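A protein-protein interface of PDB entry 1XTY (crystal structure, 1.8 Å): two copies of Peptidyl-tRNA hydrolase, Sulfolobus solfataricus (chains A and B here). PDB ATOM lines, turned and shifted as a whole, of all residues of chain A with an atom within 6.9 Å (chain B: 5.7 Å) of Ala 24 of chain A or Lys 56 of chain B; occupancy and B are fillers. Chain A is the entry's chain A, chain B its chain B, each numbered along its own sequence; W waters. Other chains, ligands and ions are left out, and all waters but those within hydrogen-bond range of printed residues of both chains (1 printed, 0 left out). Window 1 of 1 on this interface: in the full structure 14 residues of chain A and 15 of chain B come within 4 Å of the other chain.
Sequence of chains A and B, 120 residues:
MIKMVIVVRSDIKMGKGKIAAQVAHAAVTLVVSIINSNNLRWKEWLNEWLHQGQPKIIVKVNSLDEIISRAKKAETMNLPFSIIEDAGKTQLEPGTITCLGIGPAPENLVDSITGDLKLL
The side-chain amide oxygen of Gln 54 of chain B lies within hydrogen-bond range of a ring nitrogen (ND1) of His 25 of chain A. The side-chain hydroxyl of Thr 29 of chain A lies within hydrogen-bond range of the side-chain amide nitrogen of Gln 54 of chain B (3.2 Å).
The backbone carbonyl oxygen (O) of Trp 49 of chain B sits at hydrogen-bond distance from the backbone NH (N) of Gln 54 of chain B. The side-chain hydroxyl of Thr 29 of chain A sits at hydrogen-bond distance from the backbone carbonyl oxygen of His 25 of chain A (3.0 Å). The backbone carbonyl oxygen (O) of Gln 54 of chain B lies within hydrogen-bond range of the side-chain amino group (NZ) of Lys 56 of chain B (3.1 Å).
Among the printed residues, pairs that only touch across the chains: Ala 21 of chain A with Ile 58 of chain B (3.3 Å), Val 28 of chain A with Gln 54 of chain B (3.4 Å), Ala 20 of chain A with Ile 58 of chain B (3.6 Å), Ala 24 of chain A with Lys 56 of chain B (3.7 Å), Ala 27 of chain A with Val 28 of chain B (3.8 Å), Val 28 of chain A with Ala 27 of chain B (3.8 Å), His 25 of chain A with Lys 56 of chain B (3.8 Å) and Ala 20 of chain A with Val 23 of chain B (3.9 Å).
Ala 24 of chain A touches just one residue of chain B: Lys 56 (3.7 Å). Of chain A, only Ala 24 and His 25 come within 4 Å of Lys 56 of chain B. Of the printed residues of chain B, Ala 21 of chain A touches Ile 58. Printed residues of chain A within 4 Å of Val 23 of chain B: Ala 20 (3.9 Å). Lys 18 of chain A touches none of the printed residues of chain B. Ile 57 of chain B touches none of the printed residues of chain A. The nearest residue of chain A that does not touch Lys 56 of chain B is Ala 21 of chain A (4.4 Å).
Of the 15 printed residues of chain B, 6 touch a printed residue of chain A. Printed residues of chain B that touch a printed residue of chain A: Val 23, Ala 27, Val 28, Gln 54, Lys 56 and Ile 58. Hydrophobic or aromatic side chains of chain B within 4 Å of the printed part of chain A: Val 23, Ala 27, Val 28 and Ile 58. Among the printed residues, no Asp or Glu carboxylate lies within 4 Å of a Lys or Arg side-chain nitrogen of the other chain.
Ala 20 of chain A touches Val 23 of chain B, but with the chains exchanged Val 23 of chain A does not touch Ala 20 of chain B (4.1 Å). Ala 27 of chain A touches Val 28 of chain B, and with the chains exchanged Val 28 of chain A touches Ala 27 of chain B. Positions printed for both chains: 6, 20, 23, 24, 27 and 28.
Water W1 bridges the side-chain hydroxyl of Thr 29 of chain A (3.2 Å) and the side-chain amide nitrogen of Gln 54 of chain B (3.3 Å).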
ATOM      1  N   ILE A   6      -0.552  22.994  18.617  1.00  0.00           N
ATOM      2  CA  ILE A   6      -0.665  22.030  19.702  1.00  0.00           C
ATOM      3  C   ILE A   6      -0.156  20.692  19.180  1.00  0.00           C
ATOM      4  O   ILE A   6      -0.642  20.176  18.172  1.00  0.00           O
ATOM      5  CB  ILE A   6      -2.122  21.866  20.199  1.00  0.00           C
ATOM      6  CG1 ILE A   6      -2.642  23.188  20.768  1.00  0.00           C
ATOM      7  CG2 ILE A   6      -2.181  20.796  21.287  1.00  0.00           C
ATOM      8  CD1 ILE A   6      -3.200  24.133  19.735  1.00  0.00           C
ATOM      9  N   LYS A  18     -11.369  12.495  24.265  1.00  0.00           N
ATOM     10  CA  LYS A  18     -10.225  12.691  25.151  1.00  0.00           C
ATOM     11  C   LYS A  18      -9.252  13.690  24.529  1.00  0.00           C
ATOM     12  O   LYS A  18      -8.807  14.628  25.187  1.00  0.00           O
ATOM     13  CB  LYS A  18      -9.515  11.353  25.375  1.00  0.00           C
ATOM     14  CG  LYS A  18      -8.386  11.389  26.390  1.00  0.00           C
ATOM     15  CD  LYS A  18      -8.929  11.544  27.797  1.00  0.00           C
ATOM     16  CE  LYS A  18      -7.829  11.386  28.827  1.00  0.00           C
ATOM     17  NZ  LYS A  18      -8.320  11.624  30.214  1.00  0.00           N
ATOM     18  N   ILE A  19      -8.921  13.476  23.259  1.00  0.00           N
ATOM     19  CA  ILE A  19      -8.003  14.353  22.544  1.00  0.00           C
ATOM     20  C   ILE A  19      -8.496  15.796  22.552  1.00  0.00           C
ATOM     21  O   ILE A  19      -7.723  16.725  22.793  1.00  0.00           O
ATOM     22  CB  ILE A  19      -7.820  13.904  21.069  1.00  0.00           C
ATOM     23  CG1 ILE A  19      -7.033  12.593  21.020  1.00  0.00           C
ATOM     24  CG2 ILE A  19      -7.108  14.987  20.267  1.00  0.00           C
ATOM     25  CD1 ILE A  19      -6.807  12.063  19.617  1.00  0.00           C
ATOM     26  N   ALA A  20      -9.786  15.982  22.295  1.00  0.00           N
ATOM     27  CA  ALA A  20     -10.358  17.325  22.273  1.00  0.00           C
ATOM     28  C   ALA A  20     -10.189  18.019  23.623  1.00  0.00           C
ATOM     29  O   ALA A  20      -9.865  19.204  23.682  1.00  0.00           O
ATOM     30  CB  ALA A  20     -11.834  17.259  21.897  1.00  0.00           C
ATOM     31  N   ALA A  21     -10.410  17.284  24.708  1.00  0.00           N
ATOM     32  CA  ALA A  21     -10.268  17.864  26.036  1.00  0.00           C
ATOM     33  C   ALA A  21      -8.820  18.274  26.310  1.00  0.00           C
ATOM     34  O   ALA A  21      -8.568  19.360  26.839  1.00  0.00           O
ATOM     35  CB  ALA A  21     -10.745  16.871  27.098  1.00  0.00           C
ATOM     36  N   GLN A  22      -7.872  17.413  25.946  1.00  0.00           N
ATOM     37  CA  GLN A  22      -6.455  17.701  26.165  1.00  0.00           C
ATOM     38  C   GLN A  22      -5.979  18.917  25.367  1.00  0.00           C
ATOM     39  O   GLN A  22      -5.243  19.757  25.887  1.00  0.00           O
ATOM     40  CB  GLN A  22      -5.593  16.479  25.807  1.00  0.00           C
ATOM     41  CG  GLN A  22      -5.972  15.202  26.555  1.00  0.00           C
ATOM     42  CD  GLN A  22      -5.788  15.314  28.061  1.00  0.00           C
ATOM     43  OE1 GLN A  22      -6.668  14.931  28.830  1.00  0.00           O
ATOM     44  NE2 GLN A  22      -4.639  15.826  28.489  1.00  0.00           N
ATOM     45  N   VAL A  23      -6.389  19.003  24.102  1.00  0.00           N
ATOM     46  CA  VAL A  23      -6.001  20.122  23.249  1.00  0.00           C
ATOM     47  C   VAL A  23      -6.615  21.420  23.782  1.00  0.00           C
ATOM     48  O   VAL A  23      -5.970  22.470  23.781  1.00  0.00           O
ATOM     49  CB  VAL A  23      -6.448  19.878  21.781  1.00  0.00           C
ATOM     50  CG1 VAL A  23      -6.258  21.136  20.945  1.00  0.00           C
ATOM     51  CG2 VAL A  23      -5.624  18.740  21.184  1.00  0.00           C
ATOM     52  N   ALA A  24      -7.858  21.343  24.245  1.00  0.00           N
ATOM     53  CA  ALA A  24      -8.529  22.518  24.800  1.00  0.00           C
ATOM     54  C   ALA A  24      -7.808  22.947  26.079  1.00  0.00           C
ATOM     55  O   ALA A  24      -7.728  24.136  26.388  1.00  0.00           O
ATOM     56  CB  ALA A  24      -9.997  22.194  25.099  1.00  0.00           C
ATOM     57  N   HIS A  25      -7.294  21.967  26.820  1.00  0.00           N
ATOM     58  CA  HIS A  25      -6.563  22.224  28.060  1.00  0.00           C
ATOM     59  C   HIS A  25      -5.277  22.979  27.708  1.00  0.00           C
ATOM     60  O   HIS A  25      -4.916  23.962  28.358  1.00  0.00           O
ATOM     61  CB  HIS A  25      -6.222  20.888  28.741  1.00  0.00           C
ATOM     62  CG  HIS A  25      -5.797  21.015  30.173  1.00  0.00           C
ATOM     63  ND1 HIS A  25      -5.364  22.202  30.727  1.00  0.00           N
ATOM     64  CD2 HIS A  25      -5.704  20.088  31.157  1.00  0.00           C
ATOM     65  CE1 HIS A  25      -5.023  22.000  31.988  1.00  0.00           C
ATOM     66  NE2 HIS A  25      -5.219  20.725  32.274  1.00  0.00           N
ATOM     67  N   ALA A  26      -4.590  22.517  26.669  1.00  0.00           N
ATOM     68  CA  ALA A  26      -3.354  23.160  26.232  1.00  0.00           C
ATOM     69  C   ALA A  26      -3.606  24.605  25.814  1.00  0.00           C
ATOM     70  O   ALA A  26      -2.850  25.501  26.185  1.00  0.00           O
ATOM     71  CB  ALA A  26      -2.735  22.380  25.070  1.00  0.00           C
ATOM     72  N   ALA A  27      -4.675  24.836  25.054  1.00  0.00           N
ATOM     73  CA  ALA A  27      -4.993  26.180  24.582  1.00  0.00           C
ATOM     74  C   ALA A  27      -5.369  27.152  25.693  1.00  0.00           C
ATOM     75  O   ALA A  27      -4.891  28.289  25.714  1.00  0.00           O
ATOM     76  CB  ALA A  27      -6.117  26.116  23.542  1.00  0.00           C
ATOM     77  N   VAL A  28      -6.220  26.713  26.616  1.00  0.00           N
ATOM     78  CA  VAL A  28      -6.641  27.582  27.713  1.00  0.00           C
ATOM     79  C   VAL A  28      -5.475  27.926  28.637  1.00  0.00           C
ATOM     80  O   VAL A  28      -5.316  29.077  29.049  1.00  0.00           O
ATOM     81  CB  VAL A  28      -7.781  26.937  28.531  1.00  0.00           C
ATOM     82  CG1 VAL A  28      -8.089  27.777  29.766  1.00  0.00           C
ATOM     83  CG2 VAL A  28      -9.029  26.818  27.660  1.00  0.00           C
ATOM     84  N   THR A  29      -4.659  26.931  28.961  1.00  0.00           N
ATOM     85  CA  THR A  29      -3.510  27.167  29.823  1.00  0.00           C
ATOM     86  C   THR A  29      -2.570  28.200  29.195  1.00  0.00           C
ATOM     87  O   THR A  29      -2.049  29.070  29.887  1.00  0.00           O
ATOM     88  CB  THR A  29      -2.762  25.848  30.110  1.00  0.00           C
ATOM     89  OG1 THR A  29      -3.604  24.999  30.903  1.00  0.00           O
ATOM     90  CG2 THR A  29      -1.468  26.108  30.878  1.00  0.00           C
ATOM     91  N   LEU A  30      -2.357  28.112  27.885  1.00  0.00           N
ATOM     92  CA  LEU A  30      -1.496  29.072  27.197  1.00  0.00           C
ATOM     93  C   LEU A  30      -2.060  30.487  27.314  1.00  0.00           C
ATOM     94  O   LEU A  30      -1.373  31.407  27.758  1.00  0.00           O
ATOM     95  CB  LEU A  30      -1.366  28.716  25.712  1.00  0.00           C
ATOM     96  CG  LEU A  30      -0.348  27.654  25.307  1.00  0.00           C
ATOM     97  CD1 LEU A  30      -0.510  27.350  23.817  1.00  0.00           C
ATOM     98  CD2 LEU A  30       1.062  28.151  25.599  1.00  0.00           C
ATOM     99  N   ILE A  84       0.844  19.633  28.979  1.00  0.00           N
ATOM    100  CA  ILE A  84      -0.352  19.099  29.611  1.00  0.00           C
ATOM    101  C   ILE A  84      -0.217  17.646  30.058  1.00  0.00           C
ATOM    102  O   ILE A  84       0.248  16.798  29.299  1.00  0.00           O
ATOM    103  CB  ILE A  84      -1.551  19.215  28.651  1.00  0.00           C
ATOM    104  CG1 ILE A  84      -1.747  20.685  28.252  1.00  0.00           C
ATOM    105  CG2 ILE A  84      -2.800  18.645  29.297  1.00  0.00           C
ATOM    106  CD1 ILE A  84      -1.988  21.622  29.435  1.00  0.00           C
ATOM    107  N   CYS A  99       0.113  16.287  25.591  1.00  0.00           N
ATOM    108  CA  CYS A  99       0.353  17.213  24.496  1.00  0.00           C
ATOM    109  C   CYS A  99       1.107  18.461  24.928  1.00  0.00           C
ATOM    110  O   CYS A  99       1.287  18.723  26.123  1.00  0.00           O
ATOM    111  CB  CYS A  99      -0.972  17.612  23.834  1.00  0.00           C
ATOM    112  SG  CYS A  99      -2.128  18.499  24.907  1.00  0.00           S
ATOM    113  N   MET B   4     -17.117  22.983  32.539  1.00  0.00           N
ATOM    114  CA  MET B   4     -17.358  23.589  31.242  1.00  0.00           C
ATOM    115  C   MET B   4     -17.831  22.444  30.365  1.00  0.00           C
ATOM    116  O   MET B   4     -17.279  21.346  30.426  1.00  0.00           O
ATOM    117  CB  MET B   4     -16.071  24.176  30.651  1.00  0.00           C
ATOM    118  CG  MET B   4     -16.277  24.775  29.264  1.00  0.00           C
ATOM    119  SD  MET B   4     -14.768  25.296  28.430  1.00  0.00           S
ATOM    120  CE  MET B   4     -14.440  26.852  29.259  1.00  0.00           C
ATOM    121  N   VAL B   5     -18.865  22.676  29.568  1.00  0.00           N
ATOM    122  CA  VAL B   5     -19.336  21.633  28.671  1.00  0.00           C
ATOM    123  C   VAL B   5     -19.284  22.148  27.243  1.00  0.00           C
ATOM    124  O   VAL B   5     -19.601  23.301  26.978  1.00  0.00           O
ATOM    125  CB  VAL B   5     -20.784  21.198  29.004  1.00  0.00           C
ATOM    126  CG1 VAL B   5     -21.303  20.215  27.945  1.00  0.00           C
ATOM    127  CG2 VAL B   5     -20.810  20.526  30.365  1.00  0.00           C
ATOM    128  N   ILE B   6     -18.838  21.305  26.325  1.00  0.00           N
ATOM    129  CA  ILE B   6     -18.807  21.705  24.927  1.00  0.00           C
ATOM    130  C   ILE B   6     -19.635  20.674  24.180  1.00  0.00           C
ATOM    131  O   ILE B   6     -19.347  19.473  24.233  1.00  0.00           O
ATOM    132  CB  ILE B   6     -17.371  21.750  24.346  1.00  0.00           C
ATOM    133  CG1 ILE B   6     -16.531  22.795  25.081  1.00  0.00           C
ATOM    134  CG2 ILE B   6     -17.423  22.141  22.880  1.00  0.00           C
ATOM    135  CD1 ILE B   6     -15.732  22.249  26.240  1.00  0.00           C
ATOM    136  N   ALA B  20     -11.058  18.673  17.648  1.00  0.00           N
ATOM    137  CA  ALA B  20     -10.215  19.222  18.706  1.00  0.00           C
ATOM    138  C   ALA B  20     -10.057  20.730  18.548  1.00  0.00           C
ATOM    139  O   ALA B  20     -10.099  21.475  19.526  1.00  0.00           O
ATOM    140  CB  ALA B  20      -8.846  18.547  18.692  1.00  0.00           C
ATOM    141  N   VAL B  23     -13.362  22.507  19.540  1.00  0.00           N
ATOM    142  CA  VAL B  23     -13.577  22.487  20.982  1.00  0.00           C
ATOM    143  C   VAL B  23     -12.659  23.504  21.664  1.00  0.00           C
ATOM    144  O   VAL B  23     -13.087  24.217  22.565  1.00  0.00           O
ATOM    145  CB  VAL B  23     -13.340  21.070  21.562  1.00  0.00           C
ATOM    146  CG1 VAL B  23     -13.420  21.101  23.086  1.00  0.00           C
ATOM    147  CG2 VAL B  23     -14.389  20.109  21.011  1.00  0.00           C
ATOM    148  N   ALA B  24     -11.400  23.571  21.229  1.00  0.00           N
ATOM    149  CA  ALA B  24     -10.451  24.527  21.794  1.00  0.00           C
ATOM    150  C   ALA B  24     -10.913  25.954  21.496  1.00  0.00           C
ATOM    151  O   ALA B  24     -10.693  26.872  22.287  1.00  0.00           O
ATOM    152  CB  ALA B  24      -9.045  24.293  21.210  1.00  0.00           C
ATOM    153  N   ALA B  27     -13.672  26.738  24.013  1.00  0.00           N
ATOM    154  CA  ALA B  27     -13.113  26.941  25.343  1.00  0.00           C
ATOM    155  C   ALA B  27     -12.404  28.281  25.470  1.00  0.00           C
ATOM    156  O   ALA B  27     -12.620  29.008  26.438  1.00  0.00           O
ATOM    157  CB  ALA B  27     -12.152  25.801  25.697  1.00  0.00           C
ATOM    158  N   VAL B  28     -11.550  28.612  24.506  1.00  0.00           N
ATOM    159  CA  VAL B  28     -10.833  29.881  24.574  1.00  0.00           C
ATOM    160  C   VAL B  28     -11.783  31.073  24.466  1.00  0.00           C
ATOM    161  O   VAL B  28     -11.629  32.056  25.184  1.00  0.00           O
ATOM    162  CB  VAL B  28      -9.745  29.983  23.471  1.00  0.00           C
ATOM    163  CG1 VAL B  28      -9.174  31.406  23.423  1.00  0.00           C
ATOM    164  CG2 VAL B  28      -8.625  28.993  23.760  1.00  0.00           C
ATOM    165  N   TRP B  49     -12.850  27.227  38.498  1.00  0.00           N
ATOM    166  CA  TRP B  49     -12.706  26.210  37.465  1.00  0.00           C
ATOM    167  C   TRP B  49     -11.221  25.921  37.199  1.00  0.00           C
ATOM    168  O   TRP B  49     -10.813  24.766  37.102  1.00  0.00           O
ATOM    169  CB  TRP B  49     -13.390  26.701  36.189  1.00  0.00           C
ATOM    170  CG  TRP B  49     -13.324  25.751  35.029  1.00  0.00           C
ATOM    171  CD1 TRP B  49     -13.932  24.533  34.927  1.00  0.00           C
ATOM    172  CD2 TRP B  49     -12.672  25.980  33.776  1.00  0.00           C
ATOM    173  NE1 TRP B  49     -13.711  23.992  33.680  1.00  0.00           N
ATOM    174  CE2 TRP B  49     -12.940  24.860  32.953  1.00  0.00           C
ATOM    175  CE3 TRP B  49     -11.895  27.027  33.264  1.00  0.00           C
ATOM    176  CZ2 TRP B  49     -12.457  24.758  31.642  1.00  0.00           C
ATOM    177  CZ3 TRP B  49     -11.415  26.928  31.960  1.00  0.00           C
ATOM    178  CH2 TRP B  49     -11.700  25.796  31.164  1.00  0.00           C
ATOM    179  N   GLY B  53      -8.797  22.347  38.003  1.00  0.00           N
ATOM    180  CA  GLY B  53      -8.230  21.566  36.918  1.00  0.00           C
ATOM    181  C   GLY B  53      -8.904  21.698  35.568  1.00  0.00           C
ATOM    182  O   GLY B  53      -8.739  20.833  34.706  1.00  0.00           O
ATOM    183  N   GLN B  54      -9.683  22.757  35.384  1.00  0.00           N
ATOM    184  CA  GLN B  54     -10.353  22.996  34.109  1.00  0.00           C
ATOM    185  C   GLN B  54     -11.158  21.810  33.585  1.00  0.00           C
ATOM    186  O   GLN B  54     -11.090  21.505  32.395  1.00  0.00           O
ATOM    187  CB  GLN B  54      -9.319  23.343  33.041  1.00  0.00           C
ATOM    188  CG  GLN B  54      -8.564  24.616  33.230  1.00  0.00           C
ATOM    189  CD  GLN B  54      -7.535  24.796  32.133  1.00  0.00           C
ATOM    190  OE1 GLN B  54      -7.809  24.503  30.964  1.00  0.00           O
ATOM    191  NE2 GLN B  54      -6.353  25.283  32.494  1.00  0.00           N
ATOM    192  N   PRO B  55     -11.930  21.131  34.445  1.00  0.00           N
ATOM    193  CA  PRO B  55     -12.700  19.988  33.938  1.00  0.00           C
ATOM    194  C   PRO B  55     -13.656  20.327  32.796  1.00  0.00           C
ATOM    195  O   PRO B  55     -14.417  21.292  32.867  1.00  0.00           O
ATOM    196  CB  PRO B  55     -13.424  19.476  35.184  1.00  0.00           C
ATOM    197  CG  PRO B  55     -13.562  20.707  36.038  1.00  0.00           C
ATOM    198  CD  PRO B  55     -12.227  21.384  35.866  1.00  0.00           C
ATOM    199  N   LYS B  56     -13.615  19.522  31.740  1.00  0.00           N
ATOM    200  CA  LYS B  56     -14.477  19.754  30.588  1.00  0.00           C
ATOM    201  C   LYS B  56     -15.244  18.497  30.226  1.00  0.00           C
ATOM    202  O   LYS B  56     -14.691  17.398  30.233  1.00  0.00           O
ATOM    203  CB  LYS B  56     -13.651  20.189  29.376  1.00  0.00           C
ATOM    204  CG  LYS B  56     -12.830  21.454  29.563  1.00  0.00           C
ATOM    205  CD  LYS B  56     -11.928  21.686  28.355  1.00  0.00           C
ATOM    206  CE  LYS B  56     -10.954  22.835  28.575  1.00  0.00           C
ATOM    207  NZ  LYS B  56     -10.011  22.557  29.696  1.00  0.00           N
ATOM    208  N   ILE B  57     -16.524  18.659  29.921  1.00  0.00           N
ATOM    209  CA  ILE B  57     -17.349  17.533  29.519  1.00  0.00           C
ATOM    210  C   ILE B  57     -17.646  17.758  28.042  1.00  0.00           C
ATOM    211  O   ILE B  57     -18.214  18.781  27.673  1.00  0.00           O
ATOM    212  CB  ILE B  57     -18.677  17.493  30.294  1.00  0.00           C
ATOM    213  CG1 ILE B  57     -18.401  17.432  31.800  1.00  0.00           C
ATOM    214  CG2 ILE B  57     -19.493  16.268  29.861  1.00  0.00           C
ATOM    215  CD1 ILE B  57     -19.651  17.576  32.663  1.00  0.00           C
ATOM    216  N   ILE B  58     -17.249  16.815  27.200  1.00  0.00           N
ATOM    217  CA  ILE B  58     -17.487  16.950  25.776  1.00  0.00           C
ATOM    218  C   ILE B  58     -18.578  15.978  25.348  1.00  0.00           C
ATOM    219  O   ILE B  58     -18.396  14.759  25.389  1.00  0.00           O
ATOM    220  CB  ILE B  58     -16.190  16.699  24.993  1.00  0.00           C
ATOM    221  CG1 ILE B  58     -15.083  17.595  25.572  1.00  0.00           C
ATOM    222  CG2 ILE B  58     -16.404  17.004  23.512  1.00  0.00           C
ATOM    223  CD1 ILE B  58     -13.712  17.334  25.008  1.00  0.00           C
HETATM  224  O   HOH W   1      -3.696  27.034  33.316  1.00  0.00           O
